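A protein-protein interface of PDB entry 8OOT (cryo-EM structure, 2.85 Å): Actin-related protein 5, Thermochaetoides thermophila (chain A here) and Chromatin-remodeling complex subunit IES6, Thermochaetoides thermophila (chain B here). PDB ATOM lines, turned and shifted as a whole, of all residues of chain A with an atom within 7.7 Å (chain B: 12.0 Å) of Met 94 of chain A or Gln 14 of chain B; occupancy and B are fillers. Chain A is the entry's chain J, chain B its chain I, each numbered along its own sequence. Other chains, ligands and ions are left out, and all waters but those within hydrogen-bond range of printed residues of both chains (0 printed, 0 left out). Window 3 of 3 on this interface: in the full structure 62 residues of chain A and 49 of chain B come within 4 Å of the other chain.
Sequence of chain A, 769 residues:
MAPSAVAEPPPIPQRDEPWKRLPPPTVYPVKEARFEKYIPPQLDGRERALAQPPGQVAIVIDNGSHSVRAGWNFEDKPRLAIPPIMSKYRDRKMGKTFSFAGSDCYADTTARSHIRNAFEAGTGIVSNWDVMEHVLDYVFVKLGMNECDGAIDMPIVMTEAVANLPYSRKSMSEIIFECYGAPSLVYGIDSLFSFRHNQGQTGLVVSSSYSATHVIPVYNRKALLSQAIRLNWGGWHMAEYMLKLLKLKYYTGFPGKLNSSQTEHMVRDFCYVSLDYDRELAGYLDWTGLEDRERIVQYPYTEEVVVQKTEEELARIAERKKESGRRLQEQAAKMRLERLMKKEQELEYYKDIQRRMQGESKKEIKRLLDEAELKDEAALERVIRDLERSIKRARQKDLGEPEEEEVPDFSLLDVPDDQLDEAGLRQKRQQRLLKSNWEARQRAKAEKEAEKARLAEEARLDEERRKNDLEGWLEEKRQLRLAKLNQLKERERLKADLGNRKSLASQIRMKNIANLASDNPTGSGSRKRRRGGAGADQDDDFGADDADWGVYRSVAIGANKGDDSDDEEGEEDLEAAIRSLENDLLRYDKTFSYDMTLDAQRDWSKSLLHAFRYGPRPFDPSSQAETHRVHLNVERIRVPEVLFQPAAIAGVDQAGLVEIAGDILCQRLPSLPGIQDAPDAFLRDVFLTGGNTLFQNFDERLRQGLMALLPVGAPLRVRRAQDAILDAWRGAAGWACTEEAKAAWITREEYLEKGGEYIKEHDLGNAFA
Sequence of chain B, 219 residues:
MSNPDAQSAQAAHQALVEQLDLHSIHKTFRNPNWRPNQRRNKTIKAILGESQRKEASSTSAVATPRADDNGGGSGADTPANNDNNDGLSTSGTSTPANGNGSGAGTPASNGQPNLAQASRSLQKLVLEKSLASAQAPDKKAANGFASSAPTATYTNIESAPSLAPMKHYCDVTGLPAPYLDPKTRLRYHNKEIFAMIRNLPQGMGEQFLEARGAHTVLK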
ATOM      1  N   TYR A  89      25.206  -3.671  32.275  1.00  0.00           N
ATOM      2  CA  TYR A  89      24.627  -2.383  31.921  1.00  0.00           C
ATOM      3  C   TYR A  89      23.122  -2.443  32.131  1.00  0.00           C
ATOM      4  O   TYR A  89      22.529  -3.522  32.204  1.00  0.00           O
ATOM      5  CB  TYR A  89      24.958  -2.004  30.474  1.00  0.00           C
ATOM      6  CG  TYR A  89      24.339  -2.917  29.439  1.00  0.00           C
ATOM      7  CD1 TYR A  89      24.986  -4.076  29.031  1.00  0.00           C
ATOM      8  CD2 TYR A  89      23.117  -2.611  28.855  1.00  0.00           C
ATOM      9  CE1 TYR A  89      24.428  -4.907  28.082  1.00  0.00           C
ATOM     10  CE2 TYR A  89      22.552  -3.438  27.906  1.00  0.00           C
ATOM     11  CZ  TYR A  89      23.211  -4.583  27.522  1.00  0.00           C
ATOM     12  OH  TYR A  89      22.651  -5.410  26.578  1.00  0.00           O
ATOM     13  N   ARG A  90      22.511  -1.263  32.219  1.00  0.00           N
ATOM     14  CA  ARG A  90      21.060  -1.123  32.271  1.00  0.00           C
ATOM     15  C   ARG A  90      20.538  -0.765  30.885  1.00  0.00           C
ATOM     16  O   ARG A  90      20.953   0.242  30.304  1.00  0.00           O
ATOM     17  CB  ARG A  90      20.649  -0.066  33.296  1.00  0.00           C
ATOM     18  CG  ARG A  90      19.145   0.071  33.466  1.00  0.00           C
ATOM     19  CD  ARG A  90      18.784   0.926  34.673  1.00  0.00           C
ATOM     20  NE  ARG A  90      19.196   2.318  34.523  1.00  0.00           N
ATOM     21  CZ  ARG A  90      20.263   2.852  35.103  1.00  0.00           C
ATOM     22  NH1 ARG A  90      21.073   2.128  35.859  1.00  0.00           N
ATOM     23  NH2 ARG A  90      20.528   4.141  34.913  1.00  0.00           N
ATOM     24  N   ASP A  91      19.632  -1.588  30.361  1.00  0.00           N
ATOM     25  CA  ASP A  91      18.995  -1.313  29.077  1.00  0.00           C
ATOM     26  C   ASP A  91      17.937  -0.231  29.273  1.00  0.00           C
ATOM     27  O   ASP A  91      16.870  -0.490  29.837  1.00  0.00           O
ATOM     28  CB  ASP A  91      18.384  -2.593  28.510  1.00  0.00           C
ATOM     29  CG  ASP A  91      17.735  -2.391  27.149  1.00  0.00           C
ATOM     30  OD1 ASP A  91      17.726  -1.252  26.636  1.00  0.00           O
ATOM     31  OD2 ASP A  91      17.225  -3.383  26.588  1.00  0.00           O
ATOM     32  N   ARG A  92      18.238   0.984  28.807  1.00  0.00           N
ATOM     33  CA  ARG A  92      17.322   2.111  28.962  1.00  0.00           C
ATOM     34  C   ARG A  92      15.997   1.899  28.239  1.00  0.00           C
ATOM     35  O   ARG A  92      15.010   2.562  28.572  1.00  0.00           O
ATOM     36  CB  ARG A  92      17.981   3.399  28.462  1.00  0.00           C
ATOM     37  CG  ARG A  92      19.355   3.663  29.048  1.00  0.00           C
ATOM     38  CD  ARG A  92      19.327   3.608  30.568  1.00  0.00           C
ATOM     39  NE  ARG A  92      18.511   4.670  31.140  1.00  0.00           N
ATOM     40  CZ  ARG A  92      18.952   5.891  31.412  1.00  0.00           C
ATOM     41  NH1 ARG A  92      20.208   6.239  31.184  1.00  0.00           N
ATOM     42  NH2 ARG A  92      18.113   6.785  31.928  1.00  0.00           N
ATOM     43  N   LYS A  93      15.950   0.992  27.265  1.00  0.00           N
ATOM     44  CA  LYS A  93      14.715   0.666  26.568  1.00  0.00           C
ATOM     45  C   LYS A  93      13.894  -0.411  27.262  1.00  0.00           C
ATOM     46  O   LYS A  93      12.783  -0.707  26.811  1.00  0.00           O
ATOM     47  CB  LYS A  93      15.021   0.218  25.135  1.00  0.00           C
ATOM     48  CG  LYS A  93      15.751   1.256  24.303  1.00  0.00           C
ATOM     49  CD  LYS A  93      15.792   0.853  22.839  1.00  0.00           C
ATOM     50  CE  LYS A  93      16.578  -0.431  22.643  1.00  0.00           C
ATOM     51  NZ  LYS A  93      16.687  -0.794  21.204  1.00  0.00           N
ATOM     52  N   MET A  94      14.406  -1.002  28.339  1.00  0.00           N
ATOM     53  CA  MET A  94      13.694  -2.055  29.050  1.00  0.00           C
ATOM     54  C   MET A  94      13.669  -1.857  30.559  1.00  0.00           C
ATOM     55  O   MET A  94      12.829  -2.470  31.229  1.00  0.00           O
ATOM     56  CB  MET A  94      14.313  -3.423  28.721  1.00  0.00           C
ATOM     57  CG  MET A  94      13.494  -4.627  29.148  1.00  0.00           C
ATOM     58  SD  MET A  94      14.263  -6.172  28.629  1.00  0.00           S
ATOM     59  CE  MET A  94      14.052  -6.069  26.853  1.00  0.00           C
ATOM     60  N   GLY A  95      14.537  -1.014  31.112  1.00  0.00           N
ATOM     61  CA  GLY A  95      14.519  -0.682  32.520  1.00  0.00           C
ATOM     62  C   GLY A  95      15.135  -1.706  33.444  1.00  0.00           C
ATOM     63  O   GLY A  95      14.988  -1.578  34.665  1.00  0.00           O
ATOM     64  N   LYS A  96      15.819  -2.713  32.912  1.00  0.00           N
ATOM     65  CA  LYS A  96      16.416  -3.763  33.721  1.00  0.00           C
ATOM     66  C   LYS A  96      17.917  -3.794  33.473  1.00  0.00           C
ATOM     67  O   LYS A  96      18.392  -3.451  32.386  1.00  0.00           O
ATOM     68  CB  LYS A  96      15.796  -5.135  33.435  1.00  0.00           C
ATOM     69  CG  LYS A  96      16.160  -5.731  32.095  1.00  0.00           C
ATOM     70  CD  LYS A  96      15.665  -7.162  32.006  1.00  0.00           C
ATOM     71  CE  LYS A  96      14.149  -7.218  31.968  1.00  0.00           C
ATOM     72  NZ  LYS A  96      13.654  -8.615  31.836  1.00  0.00           N
ATOM     73  N   THR A  97      18.662  -4.204  34.493  1.00  0.00           N
ATOM     74  CA  THR A  97      20.076  -4.497  34.326  1.00  0.00           C
ATOM     75  C   THR A  97      20.270  -5.830  33.613  1.00  0.00           C
ATOM     76  O   THR A  97      19.570  -6.808  33.888  1.00  0.00           O
ATOM     77  CB  THR A  97      20.775  -4.515  35.685  1.00  0.00           C
ATOM     78  OG1 THR A  97      20.687  -3.215  36.282  1.00  0.00           O
ATOM     79  CG2 THR A  97      22.239  -4.883  35.534  1.00  0.00           C
ATOM     80  N   PHE A  98      21.226  -5.856  32.691  1.00  0.00           N
ATOM     81  CA  PHE A  98      21.745  -7.083  32.108  1.00  0.00           C
ATOM     82  C   PHE A  98      23.196  -7.259  32.527  1.00  0.00           C
ATOM     83  O   PHE A  98      23.937  -6.280  32.654  1.00  0.00           O
ATOM     84  CB  PHE A  98      21.643  -7.061  30.584  1.00  0.00           C
ATOM     85  CG  PHE A  98      20.248  -7.233  30.069  1.00  0.00           C
ATOM     86  CD1 PHE A  98      19.730  -8.497  29.852  1.00  0.00           C
ATOM     87  CD2 PHE A  98      19.458  -6.134  29.793  1.00  0.00           C
ATOM     88  CE1 PHE A  98      18.444  -8.661  29.378  1.00  0.00           C
ATOM     89  CE2 PHE A  98      18.174  -6.293  29.315  1.00  0.00           C
ATOM     90  CZ  PHE A  98      17.667  -7.558  29.107  1.00  0.00           C
ATOM     91  N   ARG A 112      26.595  -4.749  23.076  1.00  0.00           N
ATOM     92  CA  ARG A 112      26.875  -3.371  23.456  1.00  0.00           C
ATOM     93  C   ARG A 112      28.251  -3.176  24.073  1.00  0.00           C
ATOM     94  O   ARG A 112      28.713  -2.034  24.156  1.00  0.00           O
ATOM     95  CB  ARG A 112      25.807  -2.862  24.434  1.00  0.00           C
ATOM     96  CG  ARG A 112      24.391  -3.099  23.949  1.00  0.00           C
ATOM     97  CD  ARG A 112      24.178  -2.432  22.604  1.00  0.00           C
ATOM     98  NE  ARG A 112      22.981  -2.911  21.925  1.00  0.00           N
ATOM     99  CZ  ARG A 112      22.984  -3.513  20.743  1.00  0.00           C
ATOM    100  NH1 ARG A 112      24.114  -3.791  20.113  1.00  0.00           N
ATOM    101  NH2 ARG A 112      21.826  -3.866  20.191  1.00  0.00           N
ATOM    102  N   GLN B   7       9.764  -6.858  15.021  1.00  0.00           N
ATOM    103  CA  GLN B   7      10.278  -7.836  14.069  1.00  0.00           C
ATOM    104  C   GLN B   7      10.847  -9.052  14.793  1.00  0.00           C
ATOM    105  O   GLN B   7      11.541  -8.915  15.802  1.00  0.00           O
ATOM    106  CB  GLN B   7      11.340  -7.209  13.165  1.00  0.00           C
ATOM    107  CG  GLN B   7      11.866  -8.152  12.096  1.00  0.00           C
ATOM    108  CD  GLN B   7      12.791  -7.466  11.112  1.00  0.00           C
ATOM    109  OE1 GLN B   7      13.253  -6.350  11.350  1.00  0.00           O
ATOM    110  NE2 GLN B   7      13.062  -8.129   9.995  1.00  0.00           N
ATOM    111  N   SER B   8      10.530 -10.239  14.268  1.00  0.00           N
ATOM    112  CA  SER B   8      10.908 -11.488  14.925  1.00  0.00           C
ATOM    113  C   SER B   8      12.409 -11.564  15.178  1.00  0.00           C
ATOM    114  O   SER B   8      12.844 -12.063  16.223  1.00  0.00           O
ATOM    115  CB  SER B   8      10.449 -12.679  14.085  1.00  0.00           C
ATOM    116  OG  SER B   8      10.769 -13.903  14.722  1.00  0.00           O
ATOM    117  N   ALA B   9      13.218 -11.086  14.229  1.00  0.00           N
ATOM    118  CA  ALA B   9      14.666 -11.083  14.419  1.00  0.00           C
ATOM    119  C   ALA B   9      15.068 -10.281  15.652  1.00  0.00           C
ATOM    120  O   ALA B   9      15.944 -10.705  16.415  1.00  0.00           O
ATOM    121  CB  ALA B   9      15.357 -10.530  13.172  1.00  0.00           C
ATOM    122  N   GLN B  10      14.442  -9.122  15.863  1.00  0.00           N
ATOM    123  CA  GLN B  10      14.721  -8.349  17.069  1.00  0.00           C
ATOM    124  C   GLN B  10      14.178  -9.047  18.311  1.00  0.00           C
ATOM    125  O   GLN B  10      14.826  -9.047  19.363  1.00  0.00           O
ATOM    126  CB  GLN B  10      14.142  -6.939  16.924  1.00  0.00           C
ATOM    127  CG  GLN B  10      14.470  -5.977  18.061  1.00  0.00           C
ATOM    128  CD  GLN B  10      13.470  -6.027  19.204  1.00  0.00           C
ATOM    129  OE1 GLN B  10      12.542  -6.836  19.202  1.00  0.00           O
ATOM    130  NE2 GLN B  10      13.653  -5.154  20.186  1.00  0.00           N
ATOM    131  N   ALA B  11      12.988  -9.643  18.206  1.00  0.00           N
ATOM    132  CA  ALA B  11      12.429 -10.406  19.320  1.00  0.00           C
ATOM    133  C   ALA B  11      13.290 -11.617  19.663  1.00  0.00           C
ATOM    134  O   ALA B  11      13.514 -11.915  20.841  1.00  0.00           O
ATOM    135  CB  ALA B  11      11.003 -10.842  18.990  1.00  0.00           C
ATOM    136  N   ALA B  12      13.781 -12.326  18.645  1.00  0.00           N
ATOM    137  CA  ALA B  12      14.713 -13.427  18.874  1.00  0.00           C
ATOM    138  C   ALA B  12      16.012 -12.947  19.508  1.00  0.00           C
ATOM    139  O   ALA B  12      16.580 -13.630  20.369  1.00  0.00           O
ATOM    140  CB  ALA B  12      14.998 -14.154  17.560  1.00  0.00           C
ATOM    141  N   HIS B  13      16.503 -11.779  19.094  1.00  0.00           N
ATOM    142  CA  HIS B  13      17.671 -11.193  19.743  1.00  0.00           C
ATOM    143  C   HIS B  13      17.413 -10.885  21.213  1.00  0.00           C
ATOM    144  O   HIS B  13      18.272 -11.137  22.065  1.00  0.00           O
ATOM    145  CB  HIS B  13      18.100  -9.927  19.003  1.00  0.00           C
ATOM    146  CG  HIS B  13      19.347  -9.306  19.550  1.00  0.00           C
ATOM    147  ND1 HIS B  13      19.328  -8.363  20.555  1.00  0.00           N
ATOM    148  CD2 HIS B  13      20.649  -9.494  19.234  1.00  0.00           C
ATOM    149  CE1 HIS B  13      20.566  -7.996  20.834  1.00  0.00           C
ATOM    150  NE2 HIS B  13      21.387  -8.667  20.046  1.00  0.00           N
ATOM    151  N   GLN B  14      16.244 -10.329  21.533  1.00  0.00           N
ATOM    152  CA  GLN B  14      15.883 -10.132  22.935  1.00  0.00           C
ATOM    153  C   GLN B  14      15.781 -11.451  23.691  1.00  0.00           C
ATOM    154  O   GLN B  14      16.212 -11.545  24.847  1.00  0.00           O
ATOM    155  CB  GLN B  14      14.563  -9.367  23.031  1.00  0.00           C
ATOM    156  CG  GLN B  14      14.635  -7.917  22.575  1.00  0.00           C
ATOM    157  CD  GLN B  14      15.471  -7.040  23.491  1.00  0.00           C
ATOM    158  OE1 GLN B  14      15.972  -7.489  24.523  1.00  0.00           O
ATOM    159  NE2 GLN B  14      15.625  -5.776  23.114  1.00  0.00           N
ATOM    160  N   ALA B  15      15.214 -12.481  23.063  1.00  0.00           N
ATOM    161  CA  ALA B  15      15.132 -13.791  23.704  1.00  0.00           C
ATOM    162  C   ALA B  15      16.512 -14.370  23.998  1.00  0.00           C
ATOM    163  O   ALA B  15      16.739 -14.935  25.075  1.00  0.00           O
ATOM    164  CB  ALA B  15      14.327 -14.751  22.830  1.00  0.00           C
ATOM    165  N   LEU B  16      17.443 -14.243  23.053  1.00  0.00           N
ATOM    166  CA  LEU B  16      18.819 -14.672  23.287  1.00  0.00           C
ATOM    167  C   LEU B  16      19.497 -13.860  24.386  1.00  0.00           C
ATOM    168  O   LEU B  16      20.145 -14.421  25.277  1.00  0.00           O
ATOM    169  CB  LEU B  16      19.614 -14.578  21.985  1.00  0.00           C
ATOM    170  CG  LEU B  16      21.104 -14.902  22.073  1.00  0.00           C
ATOM    171  CD1 LEU B  16      21.314 -16.338  22.523  1.00  0.00           C
ATOM    172  CD2 LEU B  16      21.784 -14.650  20.740  1.00  0.00           C
ATOM    173  N   VAL B  17      19.363 -12.534  24.336  1.00  0.00           N
ATOM    174  CA  VAL B  17      19.937 -11.672  25.371  1.00  0.00           C
ATOM    175  C   VAL B  17      19.396 -12.019  26.755  1.00  0.00           C
ATOM    176  O   VAL B  17      20.141 -12.018  27.744  1.00  0.00           O
ATOM    177  CB  VAL B  17      19.687 -10.193  25.017  1.00  0.00           C
ATOM    178  CG1 VAL B  17      19.821  -9.309  26.243  1.00  0.00           C
ATOM    179  CG2 VAL B  17      20.649  -9.743  23.931  1.00  0.00           C
ATOM    180  N   GLU B  18      18.106 -12.338  26.851  1.00  0.00           N
ATOM    181  CA  GLU B  18      17.564 -12.833  28.114  1.00  0.00           C
ATOM    182  C   GLU B  18      18.133 -14.197  28.485  1.00  0.00           C
ATOM    183  O   GLU B  18      18.486 -14.432  29.647  1.00  0.00           O
ATOM    184  CB  GLU B  18      16.039 -12.890  28.046  1.00  0.00           C
ATOM    185  CG  GLU B  18      15.361 -11.539  28.225  1.00  0.00           C
ATOM    186  CD  GLU B  18      15.389 -11.041  29.663  1.00  0.00           C
ATOM    187  OE1 GLU B  18      16.082 -11.649  30.507  1.00  0.00           O
ATOM    188  OE2 GLU B  18      14.716 -10.031  29.951  1.00  0.00           O
ATOM    189  N   GLN B  19      18.223 -15.108  27.518  1.00  0.00           N
ATOM    190  CA  GLN B  19      18.776 -16.433  27.780  1.00  0.00           C
ATOM    191  C   GLN B  19      20.225 -16.365  28.252  1.00  0.00           C
ATOM    192  O   GLN B  19      20.650 -17.170  29.089  1.00  0.00           O
ATOM    193  CB  GLN B  19      18.657 -17.291  26.522  1.00  0.00           C
ATOM    194  CG  GLN B  19      19.223 -18.686  26.644  1.00  0.00           C
ATOM    195  CD  GLN B  19      18.903 -19.537  25.432  1.00  0.00           C
ATOM    196  OE1 GLN B  19      18.302 -19.062  24.470  1.00  0.00           O
ATOM    197  NE2 GLN B  19      19.294 -20.804  25.477  1.00  0.00           N
ATOM    198  N   LEU B  20      20.999 -15.412  27.735  1.00  0.00           N
ATOM    199  CA  LEU B  20      22.381 -15.241  28.166  1.00  0.00           C
ATOM    200  C   LEU B  20      22.530 -14.521  29.500  1.00  0.00           C
ATOM    201  O   LEU B  20      23.589 -14.636  30.126  1.00  0.00           O
ATOM    202  CB  LEU B  20      23.172 -14.485  27.098  1.00  0.00           C
ATOM    203  CG  LEU B  20      23.375 -15.248  25.790  1.00  0.00           C
ATOM    204  CD1 LEU B  20      23.940 -14.334  24.716  1.00  0.00           C
ATOM    205  CD2 LEU B  20      24.260 -16.459  26.001  1.00  0.00           C
ATOM    206  N   ASP B  21      21.518 -13.782  29.947  1.00  0.00           N
ATOM    207  CA  ASP B  21      21.678 -12.918  31.112  1.00  0.00           C
ATOM    208  C   ASP B  21      21.924 -13.730  32.379  1.00  0.00           C
ATOM    209  O   ASP B  21      21.224 -14.708  32.654  1.00  0.00           O
ATOM    210  CB  ASP B  21      20.443 -12.039  31.286  1.00  0.00           C
ATOM    211  CG  ASP B  21      20.538 -11.145  32.503  1.00  0.00           C
ATOM    212  OD1 ASP B  21      21.597 -10.511  32.692  1.00  0.00           O
ATOM    213  OD2 ASP B  21      19.558 -11.079  33.273  1.00  0.00           O
ATOM    214  N   LEU B  22      22.934 -13.315  33.147  1.00  0.00           N
ATOM    215  CA  LEU B  22      23.200 -13.845  34.479  1.00  0.00           C
ATOM    216  C   LEU B  22      22.469 -13.104  35.589  1.00  0.00           C
ATOM    217  O   LEU B  22      22.241 -13.685  36.656  1.00  0.00           O
ATOM    218  CB  LEU B  22      24.702 -13.805  34.774  1.00  0.00           C
ATOM    219  CG  LEU B  22      25.611 -14.577  33.823  1.00  0.00           C
ATOM    220  CD1 LEU B  22      27.060 -14.385  34.225  1.00  0.00           C
ATOM    221  CD2 LEU B  22      25.244 -16.049  33.812  1.00  0.00           C
ATOM    222  N   HIS B  23      22.103 -11.840  35.366  1.00  0.00           N
ATOM    223  CA  HIS B  23      21.536 -11.016  36.429  1.00  0.00           C
ATOM    224  C   HIS B  23      20.194 -11.545  36.915  1.00  0.00           C
ATOM    225  O   HIS B  23      19.872 -11.412  38.101  1.00  0.00           O
ATOM    226  CB  HIS B  23      21.387  -9.574  35.949  1.00  0.00           C
ATOM    227  CG  HIS B  23      21.206  -8.586  37.058  1.00  0.00           C
ATOM    228  ND1 HIS B  23      22.234  -8.211  37.895  1.00  0.00           N
ATOM    229  CD2 HIS B  23      20.115  -7.901  37.472  1.00  0.00           C
ATOM    230  CE1 HIS B  23      21.786  -7.332  38.774  1.00  0.00           C
ATOM    231  NE2 HIS B  23      20.503  -7.128  38.540  1.00  0.00           N
ATOM    232  N   SER B  24      19.408 -12.149  36.027  1.00  0.00           N
ATOM    233  CA  SER B  24      18.130 -12.735  36.407  1.00  0.00           C
ATOM    234  C   SER B  24      18.265 -13.936  37.336  1.00  0.00           C
ATOM    235  O   SER B  24      17.256 -14.370  37.901  1.00  0.00           O
ATOM    236  CB  SER B  24      17.355 -13.149  35.155  1.00  0.00           C
ATOM    237  OG  SER B  24      17.139 -12.040  34.300  1.00  0.00           O
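N of His 23 of chain B is in hydrogen-bond range of OD1 of Asp 21 of chain B. OG of Ser 24 of chain B is in hydrogen-bond range of OD2 of Asp 21 of chain B, at 2.8 Å. The backbone NH of Phe 98 of chain A lies within hydrogen-bond range of the backbone carbonyl oxygen of Tyr 89 of chain A (2.7 Å). The backbone carbonyl oxygen of Lys 96 of chain A sits at hydrogen-bond distance from the backbone NH of Asp 91 of chain A (3.0 Å).
NZ of Lys 96 of chain A lies within salt-bridge range of OE2 of Glu 18 of chain B.
Of the 18 printed residues of chain B, 5 touch a printed residue of chain A. Printed residues of chain B that touch a printed residue of chain A: Gln 14, Val 17, Glu 18, Asp 21 and His 23. Hydrophobic or aromatic side chains of chain B within 4 Å of the printed part of chain A: Val 17 and His 23. Of the 11 printed residues of chain A, 4 touch a printed residue of chain B. Printed residues of chain A that touch a printed residue of chain B: Met 94, Lys 96, Thr 97 and Phe 98.
No residue of chain B comes within 4 Å of Asp 91 of chain A. No residue of chain B comes within 4 Å of Gly 95 of chain A. Of the printed residues of chain B, Thr 97 of chain A touches His 23 (3.8 Å). Printed residues of chain A within 4 Å of Val 17 of chain B: Phe 98. Of the printed residues of chain A, Asp 21 of chain B touches Phe 98 (3.5 Å). Ala 9 of chain B touches none of the printed residues of chain A. Ala 12 of chain B touches none of the printed residues of chain A. The nearest printed residue of chain A that does not touch Glu 18 of chain B is Met 94 of chain A (4.1 Å).
Among the printed residues, merely in contact across the chains: Met 94 of chain A with Gln 14 of chain B (3.3 Å), Phe 98 of chain A with Asp 21 of chain B (3.5 Å), Phe 98 of chain A with Val 17 of chain B (3.5 Å), Thr 97 of chain A with His 23 of chain B (3.8 Å) and Phe 98 of chain A with Glu 18 of chain B (3.9 Å).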
